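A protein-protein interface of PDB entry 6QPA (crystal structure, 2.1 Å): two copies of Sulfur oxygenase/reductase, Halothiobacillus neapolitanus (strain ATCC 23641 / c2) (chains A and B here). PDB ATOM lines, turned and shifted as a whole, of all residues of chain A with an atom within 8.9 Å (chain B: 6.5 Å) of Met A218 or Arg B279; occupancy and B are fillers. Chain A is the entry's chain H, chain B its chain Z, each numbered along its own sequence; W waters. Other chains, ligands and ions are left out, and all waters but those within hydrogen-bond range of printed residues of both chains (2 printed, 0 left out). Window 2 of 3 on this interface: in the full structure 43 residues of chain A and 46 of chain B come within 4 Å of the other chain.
No position is printed for both chains. Of the 5 pairs that touch across the chains among the printed residues, none has its exchanged pair printed and touching as well.
Water W1 bridges the side-chain hydroxyl of Ser A222 and the guanidinium group of Arg B279. Water W2 lies within hydrogen-bond range of OE1 of Glu A215 (2.9 Å), NE of Arg B279 (3.1 Å) and NE2 of Gln B280 (3.4 Å).
The side-chain sulfur (SD) of Met A218 sits close to the side-chain amide oxygen (OD1) of Asn B283 (3.8 Å).
Among the printed residues, merely in contact across the chains: Pro A214 with Asn B283, Pro A214 with Leu B287, Met A218 with Met B273 and Met A218 with Arg B279.
Printed residues of chain B that touch a printed residue of chain A: Met B273, Arg B279, Asn B283 and Leu B287. Printed residues of chain A that touch a printed residue of chain B: Pro A214 and Met A218. Among the printed residues, no Asp or Glu carboxylate lies within 4 Å of a Lys or Arg side-chain nitrogen of the other chain.
O of Met A218 sits at hydrogen-bond distance from OG of Ser A222 (2.7 Å). O of Met B273 is in hydrogen-bond range of NH1 of Arg B279 (3.0 Å). The backbone carbonyl oxygen (O) of Arg B279 sits close to the side-chain amide oxygen (OD1) of Asn B283 (3.4 Å). The backbone carbonyl oxygen (O) of His B282 sits at hydrogen-bond distance from the backbone NH (N) of Leu B287, 2.9 Å away.
Of the printed residues of chain B, Pro A214 touches Asn B283 (3.4 Å) and Leu B287 (3.9 Å). Ala A217 touches none of the printed residues of chain B. Met A218 touches just these residues of chain B: Met B273, Arg B279 and Asn B283. Printed residues of chain A within 4 Å of Met B273: Met A218 (3.5 Å). Asp B275 touches none of the printed residues of chain A. Of chain A, only Met A218 (3.5 Å) comes within 4 Å of Arg B279. No residue of chain A comes within 4 Å of Gln B280. Of the printed residues of chain A, Asn B283 touches Pro A214 (3.4 Å) and Met A218 (3.7 Å). Printed residues of chain A within 4 Å of Leu B287: Pro A214. The nearest printed residue of chain A that does not touch Leu B287 is Ala A217 (4.7 Å).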
ATOM      1  N   PHE A 100     -34.486   5.195 -19.796  1.00  0.00           N
ATOM      2  CA  PHE A 100     -33.368   4.267 -19.916  1.00  0.00           C
ATOM      3  C   PHE A 100     -32.602   4.160 -18.602  1.00  0.00           C
ATOM      4  O   PHE A 100     -32.231   3.056 -18.181  1.00  0.00           O
ATOM      5  CB  PHE A 100     -32.409   4.671 -21.043  1.00  0.00           C
ATOM      6  CG  PHE A 100     -31.236   3.708 -21.183  1.00  0.00           C
ATOM      7  CD1 PHE A 100     -31.363   2.529 -21.910  1.00  0.00           C
ATOM      8  CD2 PHE A 100     -30.032   3.953 -20.527  1.00  0.00           C
ATOM      9  CE1 PHE A 100     -30.297   1.630 -22.011  1.00  0.00           C
ATOM     10  CE2 PHE A 100     -28.965   3.067 -20.618  1.00  0.00           C
ATOM     11  CZ  PHE A 100     -29.093   1.908 -21.362  1.00  0.00           C
ATOM     12  N   PHE A 210     -37.677  -2.404 -25.651  1.00  0.00           N
ATOM     13  CA  PHE A 210     -36.222  -2.363 -25.598  1.00  0.00           C
ATOM     14  C   PHE A 210     -35.575  -3.001 -26.831  1.00  0.00           C
ATOM     15  O   PHE A 210     -34.495  -3.592 -26.742  1.00  0.00           O
ATOM     16  CB  PHE A 210     -35.728  -3.035 -24.308  1.00  0.00           C
ATOM     17  CG  PHE A 210     -34.506  -2.402 -23.729  1.00  0.00           C
ATOM     18  CD1 PHE A 210     -34.558  -1.114 -23.227  1.00  0.00           C
ATOM     19  CD2 PHE A 210     -33.308  -3.095 -23.672  1.00  0.00           C
ATOM     20  CE1 PHE A 210     -33.434  -0.523 -22.686  1.00  0.00           C
ATOM     21  CE2 PHE A 210     -32.176  -2.511 -23.125  1.00  0.00           C
ATOM     22  CZ  PHE A 210     -32.240  -1.227 -22.634  1.00  0.00           C
ATOM     23  N   LEU A 212     -33.848  -2.094 -29.927  1.00  0.00           N
ATOM     24  CA  LEU A 212     -33.139  -1.009 -30.555  1.00  0.00           C
ATOM     25  C   LEU A 212     -32.512  -1.484 -31.859  1.00  0.00           C
ATOM     26  O   LEU A 212     -32.577  -2.659 -32.222  1.00  0.00           O
ATOM     27  CB  LEU A 212     -32.087  -0.470 -29.586  1.00  0.00           C
ATOM     28  CG  LEU A 212     -32.681  -0.157 -28.224  1.00  0.00           C
ATOM     29  CD1 LEU A 212     -31.612   0.418 -27.292  1.00  0.00           C
ATOM     30  CD2 LEU A 212     -33.844   0.830 -28.398  1.00  0.00           C
ATOM     31  N   ASP A 213     -31.918  -0.548 -32.586  1.00  0.00           N
ATOM     32  CA  ASP A 213     -31.037  -0.894 -33.680  1.00  0.00           C
ATOM     33  C   ASP A 213     -29.807  -1.614 -33.115  1.00  0.00           C
ATOM     34  O   ASP A 213     -29.555  -1.573 -31.911  1.00  0.00           O
ATOM     35  CB  ASP A 213     -30.606   0.369 -34.406  1.00  0.00           C
ATOM     36  CG  ASP A 213     -29.706   1.199 -33.554  1.00  0.00           C
ATOM     37  OD1 ASP A 213     -30.166   1.637 -32.485  1.00  0.00           O
ATOM     38  OD2 ASP A 213     -28.524   1.341 -33.906  1.00  0.00           O
ATOM     39  N   PRO A 214     -29.021  -2.283 -33.960  1.00  0.00           N
ATOM     40  CA  PRO A 214     -27.899  -3.067 -33.409  1.00  0.00           C
ATOM     41  C   PRO A 214     -26.905  -2.242 -32.604  1.00  0.00           C
ATOM     42  O   PRO A 214     -26.492  -2.669 -31.513  1.00  0.00           O
ATOM     43  CB  PRO A 214     -27.258  -3.682 -34.660  1.00  0.00           C
ATOM     44  CG  PRO A 214     -28.434  -3.805 -35.639  1.00  0.00           C
ATOM     45  CD  PRO A 214     -29.242  -2.552 -35.393  1.00  0.00           C
ATOM     46  N   GLU A 215     -26.543  -1.049 -33.080  1.00  0.00           N
ATOM     47  CA  GLU A 215     -25.546  -0.272 -32.351  1.00  0.00           C
ATOM     48  C   GLU A 215     -26.108   0.215 -31.019  1.00  0.00           C
ATOM     49  O   GLU A 215     -25.420   0.182 -29.992  1.00  0.00           O
ATOM     50  CB  GLU A 215     -25.046   0.892 -33.206  1.00  0.00           C
ATOM     51  CG  GLU A 215     -23.753   1.460 -32.647  1.00  0.00           C
ATOM     52  CD  GLU A 215     -22.634   0.402 -32.618  1.00  0.00           C
ATOM     53  OE1 GLU A 215     -22.654  -0.519 -33.474  1.00  0.00           O
ATOM     54  OE2 GLU A 215     -21.765   0.463 -31.712  1.00  0.00           O
ATOM     55  N   GLY A 216     -27.374   0.619 -31.008  1.00  0.00           N
ATOM     56  CA  GLY A 216     -28.009   0.963 -29.752  1.00  0.00           C
ATOM     57  C   GLY A 216     -28.062  -0.207 -28.789  1.00  0.00           C
ATOM     58  O   GLY A 216     -27.874  -0.035 -27.583  1.00  0.00           O
ATOM     59  N   ALA A 217     -28.320  -1.414 -29.308  1.00  0.00           N
ATOM     60  CA  ALA A 217     -28.348  -2.593 -28.453  1.00  0.00           C
ATOM     61  C   ALA A 217     -27.001  -2.807 -27.778  1.00  0.00           C
ATOM     62  O   ALA A 217     -26.941  -3.172 -26.596  1.00  0.00           O
ATOM     63  CB  ALA A 217     -28.740  -3.842 -29.261  1.00  0.00           C
ATOM     64  N   MET A 218     -25.912  -2.611 -28.529  1.00  0.00           N
ATOM     65  CA  MET A 218     -24.576  -2.726 -27.955  1.00  0.00           C
ATOM     66  C   MET A 218     -24.352  -1.668 -26.882  1.00  0.00           C
ATOM     67  O   MET A 218     -23.877  -1.973 -25.783  1.00  0.00           O
ATOM     68  CB  MET A 218     -23.500  -2.615 -29.043  1.00  0.00           C
ATOM     69  CG  MET A 218     -23.590  -3.653 -30.163  1.00  0.00           C
ATOM     70  SD  MET A 218     -23.705  -5.366 -29.630  1.00  0.00           S
ATOM     71  CE  MET A 218     -22.294  -5.477 -28.549  1.00  0.00           C
ATOM     72  N   LYS A 219     -24.659  -0.404 -27.189  1.00  0.00           N
ATOM     73  CA  LYS A 219     -24.430   0.628 -26.184  1.00  0.00           C
ATOM     74  C   LYS A 219     -25.314   0.431 -24.962  1.00  0.00           C
ATOM     75  O   LYS A 219     -24.897   0.769 -23.846  1.00  0.00           O
ATOM     76  CB  LYS A 219     -24.604   2.030 -26.776  1.00  0.00           C
ATOM     77  CG  LYS A 219     -23.442   2.470 -27.658  1.00  0.00           C
ATOM     78  CD  LYS A 219     -23.569   3.930 -28.046  1.00  0.00           C
ATOM     79  CE  LYS A 219     -22.293   4.462 -28.688  1.00  0.00           C
ATOM     80  NZ  LYS A 219     -21.180   4.573 -27.700  1.00  0.00           N
ATOM     81  N   ALA A 220     -26.512  -0.150 -25.140  1.00  0.00           N
ATOM     82  CA  ALA A 220     -27.427  -0.343 -24.013  1.00  0.00           C
ATOM     83  C   ALA A 220     -26.795  -1.174 -22.904  1.00  0.00           C
ATOM     84  O   ALA A 220     -27.113  -0.981 -21.726  1.00  0.00           O
ATOM     85  CB  ALA A 220     -28.717  -1.021 -24.476  1.00  0.00           C
ATOM     86  N   VAL A 221     -25.927  -2.121 -23.253  1.00  0.00           N
ATOM     87  CA  VAL A 221     -25.262  -2.946 -22.253  1.00  0.00           C
ATOM     88  C   VAL A 221     -23.830  -2.492 -22.000  1.00  0.00           C
ATOM     89  O   VAL A 221     -23.101  -3.147 -21.252  1.00  0.00           O
ATOM     90  CB  VAL A 221     -25.317  -4.439 -22.634  1.00  0.00           C
ATOM     91  CG1 VAL A 221     -26.725  -4.973 -22.448  1.00  0.00           C
ATOM     92  CG2 VAL A 221     -24.830  -4.670 -24.069  1.00  0.00           C
ATOM     93  N   SER A 222     -23.411  -1.385 -22.611  1.00  0.00           N
ATOM     94  CA  SER A 222     -22.112  -0.775 -22.372  1.00  0.00           C
ATOM     95  C   SER A 222     -22.174   0.314 -21.309  1.00  0.00           C
ATOM     96  O   SER A 222     -21.279   1.161 -21.239  1.00  0.00           O
ATOM     97  CB  SER A 222     -21.574  -0.188 -23.676  1.00  0.00           C
ATOM     98  OG  SER A 222     -21.519  -1.160 -24.699  1.00  0.00           O
ATOM     99  N   THR A 223     -23.240   0.333 -20.519  1.00  0.00           N
ATOM    100  CA  THR A 223     -23.499   1.380 -19.547  1.00  0.00           C
ATOM    101  C   THR A 223     -24.304   0.778 -18.404  1.00  0.00           C
ATOM    102  O   THR A 223     -24.940  -0.273 -18.549  1.00  0.00           O
ATOM    103  CB  THR A 223     -24.250   2.561 -20.204  1.00  0.00           C
ATOM    104  OG1 THR A 223     -24.582   3.543 -19.227  1.00  0.00           O
ATOM    105  CG2 THR A 223     -25.523   2.095 -20.877  1.00  0.00           C
ATOM    106  N   ASN A 227     -25.235   6.479 -19.580  1.00  0.00           N
ATOM    107  CA  ASN A 227     -24.827   6.806 -20.943  1.00  0.00           C
ATOM    108  C   ASN A 227     -25.712   6.049 -21.921  1.00  0.00           C
ATOM    109  O   ASN A 227     -25.310   5.011 -22.467  1.00  0.00           O
ATOM    110  CB  ASN A 227     -23.343   6.517 -21.152  1.00  0.00           C
ATOM    111  CG  ASN A 227     -22.478   7.436 -20.320  1.00  0.00           C
ATOM    112  OD1 ASN A 227     -22.378   8.636 -20.591  1.00  0.00           O
ATOM    113  ND2 ASN A 227     -21.865   6.883 -19.283  1.00  0.00           N
ATOM    114  N   PRO A 228     -26.918   6.554 -22.176  1.00  0.00           N
ATOM    115  CA  PRO A 228     -27.888   5.807 -22.980  1.00  0.00           C
ATOM    116  C   PRO A 228     -27.463   5.734 -24.434  1.00  0.00           C
ATOM    117  O   PRO A 228     -26.698   6.582 -24.919  1.00  0.00           O
ATOM    118  CB  PRO A 228     -29.179   6.628 -22.828  1.00  0.00           C
ATOM    119  CG  PRO A 228     -28.688   8.045 -22.591  1.00  0.00           C
ATOM    120  CD  PRO A 228     -27.426   7.883 -21.773  1.00  0.00           C
ATOM    121  N   PRO A 229     -27.960   4.744 -25.167  1.00  0.00           N
ATOM    122  CA  PRO A 229     -27.806   4.761 -26.623  1.00  0.00           C
ATOM    123  C   PRO A 229     -28.636   5.884 -27.228  1.00  0.00           C
ATOM    124  O   PRO A 229     -29.510   6.464 -26.582  1.00  0.00           O
ATOM    125  CB  PRO A 229     -28.347   3.399 -27.049  1.00  0.00           C
ATOM    126  CG  PRO A 229     -29.350   3.064 -25.987  1.00  0.00           C
ATOM    127  CD  PRO A 229     -28.774   3.608 -24.705  1.00  0.00           C
ATOM    128  N   HIS B 271     -19.291 -13.897 -27.600  1.00  0.00           N
ATOM    129  CA  HIS B 271     -18.419 -13.448 -28.680  1.00  0.00           C
ATOM    130  C   HIS B 271     -19.131 -12.535 -29.679  1.00  0.00           C
ATOM    131  O   HIS B 271     -18.455 -11.762 -30.370  1.00  0.00           O
ATOM    132  CB  HIS B 271     -17.801 -14.647 -29.416  1.00  0.00           C
ATOM    133  CG  HIS B 271     -16.580 -15.196 -28.737  1.00  0.00           C
ATOM    134  ND1 HIS B 271     -16.610 -15.723 -27.466  1.00  0.00           N
ATOM    135  CD2 HIS B 271     -15.293 -15.287 -29.151  1.00  0.00           C
ATOM    136  CE1 HIS B 271     -15.393 -16.112 -27.123  1.00  0.00           C
ATOM    137  NE2 HIS B 271     -14.577 -15.863 -28.131  1.00  0.00           N
ATOM    138  N   VAL B 272     -20.462 -12.609 -29.800  1.00  0.00           N
ATOM    139  CA  VAL B 272     -21.145 -11.673 -30.690  1.00  0.00           C
ATOM    140  C   VAL B 272     -21.087 -10.258 -30.150  1.00  0.00           C
ATOM    141  O   VAL B 272     -21.429  -9.314 -30.861  1.00  0.00           O
ATOM    142  CB  VAL B 272     -22.609 -12.059 -30.978  1.00  0.00           C
ATOM    143  CG1 VAL B 272     -22.692 -13.473 -31.601  1.00  0.00           C
ATOM    144  CG2 VAL B 272     -23.466 -11.913 -29.722  1.00  0.00           C
ATOM    145  N   MET B 273     -20.630 -10.087 -28.916  1.00  0.00           N
ATOM    146  CA  MET B 273     -20.439  -8.765 -28.350  1.00  0.00           C
ATOM    147  C   MET B 273     -18.975  -8.416 -28.130  1.00  0.00           C
ATOM    148  O   MET B 273     -18.616  -7.262 -28.299  1.00  0.00           O
ATOM    149  CB  MET B 273     -21.208  -8.645 -27.026  1.00  0.00           C
ATOM    150  CG  MET B 273     -22.731  -8.683 -27.190  1.00  0.00           C
ATOM    151  SD  MET B 273     -23.628  -8.523 -25.626  1.00  0.00           S
ATOM    152  CE  MET B 273     -23.197 -10.045 -24.764  1.00  0.00           C
ATOM    153  N   VAL B 274     -18.090  -9.379 -27.862  1.00  0.00           N
ATOM    154  CA  VAL B 274     -16.730  -9.021 -27.487  1.00  0.00           C
ATOM    155  C   VAL B 274     -15.707  -9.369 -28.555  1.00  0.00           C
ATOM    156  O   VAL B 274     -14.504  -9.210 -28.310  1.00  0.00           O
ATOM    157  CB  VAL B 274     -16.341  -9.635 -26.129  1.00  0.00           C
ATOM    158  CG1 VAL B 274     -17.293  -9.125 -25.075  1.00  0.00           C
ATOM    159  CG2 VAL B 274     -16.310 -11.189 -26.183  1.00  0.00           C
ATOM    160  N   ASP B 275     -16.126  -9.848 -29.723  1.00  0.00           N
ATOM    161  CA  ASP B 275     -15.225  -9.973 -30.862  1.00  0.00           C
ATOM    162  C   ASP B 275     -15.703  -9.040 -31.967  1.00  0.00           C
ATOM    163  O   ASP B 275     -16.825  -9.189 -32.459  1.00  0.00           O
ATOM    164  CB  ASP B 275     -15.133 -11.421 -31.360  1.00  0.00           C
ATOM    165  CG  ASP B 275     -14.185 -11.566 -32.537  1.00  0.00           C
ATOM    166  OD1 ASP B 275     -14.565 -11.207 -33.666  1.00  0.00           O
ATOM    167  OD2 ASP B 275     -13.025 -11.975 -32.328  1.00  0.00           O
ATOM    168  N   TYR B 276     -14.838  -8.104 -32.372  1.00  0.00           N
ATOM    169  CA  TYR B 276     -15.258  -7.043 -33.289  1.00  0.00           C
ATOM    170  C   TYR B 276     -15.798  -7.620 -34.591  1.00  0.00           C
ATOM    171  O   TYR B 276     -16.861  -7.211 -35.083  1.00  0.00           O
ATOM    172  CB  TYR B 276     -14.090  -6.099 -33.578  1.00  0.00           C
ATOM    173  CG  TYR B 276     -14.468  -5.037 -34.575  1.00  0.00           C
ATOM    174  CD1 TYR B 276     -15.077  -3.863 -34.155  1.00  0.00           C
ATOM    175  CD2 TYR B 276     -14.249  -5.223 -35.941  1.00  0.00           C
ATOM    176  CE1 TYR B 276     -15.447  -2.900 -35.056  1.00  0.00           C
ATOM    177  CE2 TYR B 276     -14.637  -4.261 -36.865  1.00  0.00           C
ATOM    178  CZ  TYR B 276     -15.236  -3.108 -36.407  1.00  0.00           C
ATOM    179  OH  TYR B 276     -15.615  -2.141 -37.285  1.00  0.00           O
ATOM    180  N   GLU B 277     -15.077  -8.580 -35.158  1.00  0.00           N
ATOM    181  CA  GLU B 277     -15.447  -9.106 -36.463  1.00  0.00           C
ATOM    182  C   GLU B 277     -16.772  -9.854 -36.387  1.00  0.00           C
ATOM    183  O   GLU B 277     -17.651  -9.642 -37.227  1.00  0.00           O
ATOM    184  CB  GLU B 277     -14.319  -9.976 -37.005  1.00  0.00           C
ATOM    185  CG  GLU B 277     -14.604 -10.583 -38.361  1.00  0.00           C
ATOM    186  CD  GLU B 277     -13.442 -11.409 -38.854  1.00  0.00           C
ATOM    187  OE1 GLU B 277     -13.345 -12.587 -38.451  1.00  0.00           O
ATOM    188  OE2 GLU B 277     -12.614 -10.870 -39.622  1.00  0.00           O
ATOM    189  N   LEU B 278     -16.939 -10.727 -35.381  1.00  0.00           N
ATOM    190  CA  LEU B 278     -18.217 -11.424 -35.222  1.00  0.00           C
ATOM    191  C   LEU B 278     -19.343 -10.451 -34.913  1.00  0.00           C
ATOM    192  O   LEU B 278     -20.481 -10.623 -35.379  1.00  0.00           O
ATOM    193  CB  LEU B 278     -18.128 -12.481 -34.119  1.00  0.00           C
ATOM    194  CG  LEU B 278     -19.434 -13.272 -33.976  1.00  0.00           C
ATOM    195  CD1 LEU B 278     -19.746 -13.969 -35.305  1.00  0.00           C
ATOM    196  CD2 LEU B 278     -19.393 -14.305 -32.822  1.00  0.00           C
ATOM    197  N   ARG B 279     -19.035  -9.416 -34.131  1.00  0.00           N
ATOM    198  CA  ARG B 279     -20.019  -8.399 -33.782  1.00  0.00           C
ATOM    199  C   ARG B 279     -20.578  -7.712 -35.026  1.00  0.00           C
ATOM    200  O   ARG B 279     -21.790  -7.497 -35.123  1.00  0.00           O
ATOM    201  CB  ARG B 279     -19.373  -7.393 -32.837  1.00  0.00           C
ATOM    202  CG  ARG B 279     -20.212  -6.257 -32.374  1.00  0.00           C
ATOM    203  CD  ARG B 279     -19.481  -5.665 -31.192  1.00  0.00           C
ATOM    204  NE  ARG B 279     -19.880  -4.303 -30.910  1.00  0.00           N
ATOM    205  CZ  ARG B 279     -19.600  -3.698 -29.768  1.00  0.00           C
ATOM    206  NH1 ARG B 279     -18.939  -4.369 -28.824  1.00  0.00           N
ATOM    207  NH2 ARG B 279     -19.986  -2.443 -29.567  1.00  0.00           N
ATOM    208  N   GLN B 280     -19.717  -7.378 -35.995  1.00  0.00           N
ATOM    209  CA  GLN B 280     -20.220  -6.790 -37.235  1.00  0.00           C
ATOM    210  C   GLN B 280     -21.091  -7.782 -37.997  1.00  0.00           C
ATOM    211  O   GLN B 280     -22.155  -7.410 -38.498  1.00  0.00           O
ATOM    212  CB  GLN B 280     -19.068  -6.303 -38.120  1.00  0.00           C
ATOM    213  CG  GLN B 280     -18.127  -5.316 -37.432  1.00  0.00           C
ATOM    214  CD  GLN B 280     -18.859  -4.256 -36.614  1.00  0.00           C
ATOM    215  OE1 GLN B 280     -19.714  -3.528 -37.125  1.00  0.00           O
ATOM    216  NE2 GLN B 280     -18.520  -4.170 -35.331  1.00  0.00           N
ATOM    217  N   ILE B 281     -20.671  -9.049 -38.076  1.00  0.00           N
ATOM    218  CA  ILE B 281     -21.471 -10.063 -38.773  1.00  0.00           C
ATOM    219  C   ILE B 281     -22.847 -10.207 -38.130  1.00  0.00           C
ATOM    220  O   ILE B 281     -23.878 -10.213 -38.813  1.00  0.00           O
ATOM    221  CB  ILE B 281     -20.720 -11.409 -38.800  1.00  0.00           C
ATOM    222  CG1 ILE B 281     -19.482 -11.328 -39.699  1.00  0.00           C
ATOM    223  CG2 ILE B 281     -21.655 -12.594 -39.177  1.00  0.00           C
ATOM    224  CD1 ILE B 281     -18.530 -12.507 -39.504  1.00  0.00           C
ATOM    225  N   HIS B 282     -22.880 -10.324 -36.803  1.00  0.00           N
ATOM    226  CA  HIS B 282     -24.125 -10.592 -36.086  1.00  0.00           C
ATOM    227  C   HIS B 282     -25.018  -9.359 -36.042  1.00  0.00           C
ATOM    228  O   HIS B 282     -26.250  -9.464 -36.150  1.00  0.00           O
ATOM    229  CB  HIS B 282     -23.797 -11.073 -34.663  1.00  0.00           C
ATOM    230  CG  HIS B 282     -24.989 -11.509 -33.868  1.00  0.00           C
ATOM    231  ND1 HIS B 282     -25.435 -10.824 -32.758  1.00  0.00           N
ATOM    232  CD2 HIS B 282     -25.794 -12.593 -33.990  1.00  0.00           C
ATOM    233  CE1 HIS B 282     -26.478 -11.451 -32.245  1.00  0.00           C
ATOM    234  NE2 HIS B 282     -26.723 -12.521 -32.981  1.00  0.00           N
ATOM    235  N   ASN B 283     -24.422  -8.190 -35.821  1.00  0.00           N
ATOM    236  CA  ASN B 283     -25.208  -6.959 -35.810  1.00  0.00           C
ATOM    237  C   ASN B 283     -25.928  -6.764 -37.136  1.00  0.00           C
ATOM    238  O   ASN B 283     -27.140  -6.535 -37.170  1.00  0.00           O
ATOM    239  CB  ASN B 283     -24.307  -5.758 -35.520  1.00  0.00           C
ATOM    240  CG  ASN B 283     -23.964  -5.621 -34.032  1.00  0.00           C
ATOM    241  OD1 ASN B 283     -24.354  -6.449 -33.206  1.00  0.00           O
ATOM    242  ND2 ASN B 283     -23.219  -4.588 -33.700  1.00  0.00           N
ATOM    243  N   ASN B 284     -25.193  -6.851 -38.243  1.00  0.00           N
ATOM    244  CA  ASN B 284     -25.792  -6.537 -39.535  1.00  0.00           C
ATOM    245  C   ASN B 284     -26.584  -7.697 -40.115  1.00  0.00           C
ATOM    246  O   ASN B 284     -27.575  -7.465 -40.816  1.00  0.00           O
ATOM    247  CB  ASN B 284     -24.720  -6.069 -40.521  1.00  0.00           C
ATOM    248  CG  ASN B 284     -24.062  -4.749 -40.082  1.00  0.00           C
ATOM    249  OD1 ASN B 284     -24.740  -3.849 -39.614  1.00  0.00           O
ATOM    250  ND2 ASN B 284     -22.761  -4.636 -40.257  1.00  0.00           N
ATOM    251  N   LEU B 287     -29.124  -9.025 -35.882  1.00  0.00           N
ATOM    252  CA  LEU B 287     -29.832  -8.056 -35.036  1.00  0.00           C
ATOM    253  C   LEU B 287     -30.611  -7.039 -35.864  1.00  0.00           C
ATOM    254  O   LEU B 287     -31.689  -6.600 -35.453  1.00  0.00           O
ATOM    255  CB  LEU B 287     -28.857  -7.332 -34.091  1.00  0.00           C
ATOM    256  CG  LEU B 287     -28.141  -8.195 -33.018  1.00  0.00           C
ATOM    257  CD1 LEU B 287     -27.340  -7.336 -32.054  1.00  0.00           C
ATOM    258  CD2 LEU B 287     -29.112  -9.006 -32.234  1.00  0.00           C
HETATM  259  O   HOH W   1     -20.781  -0.276 -27.108  1.00  0.00           O
HETATM  260  O   HOH W   2     -20.358  -2.259 -33.208  1.00  0.00           O
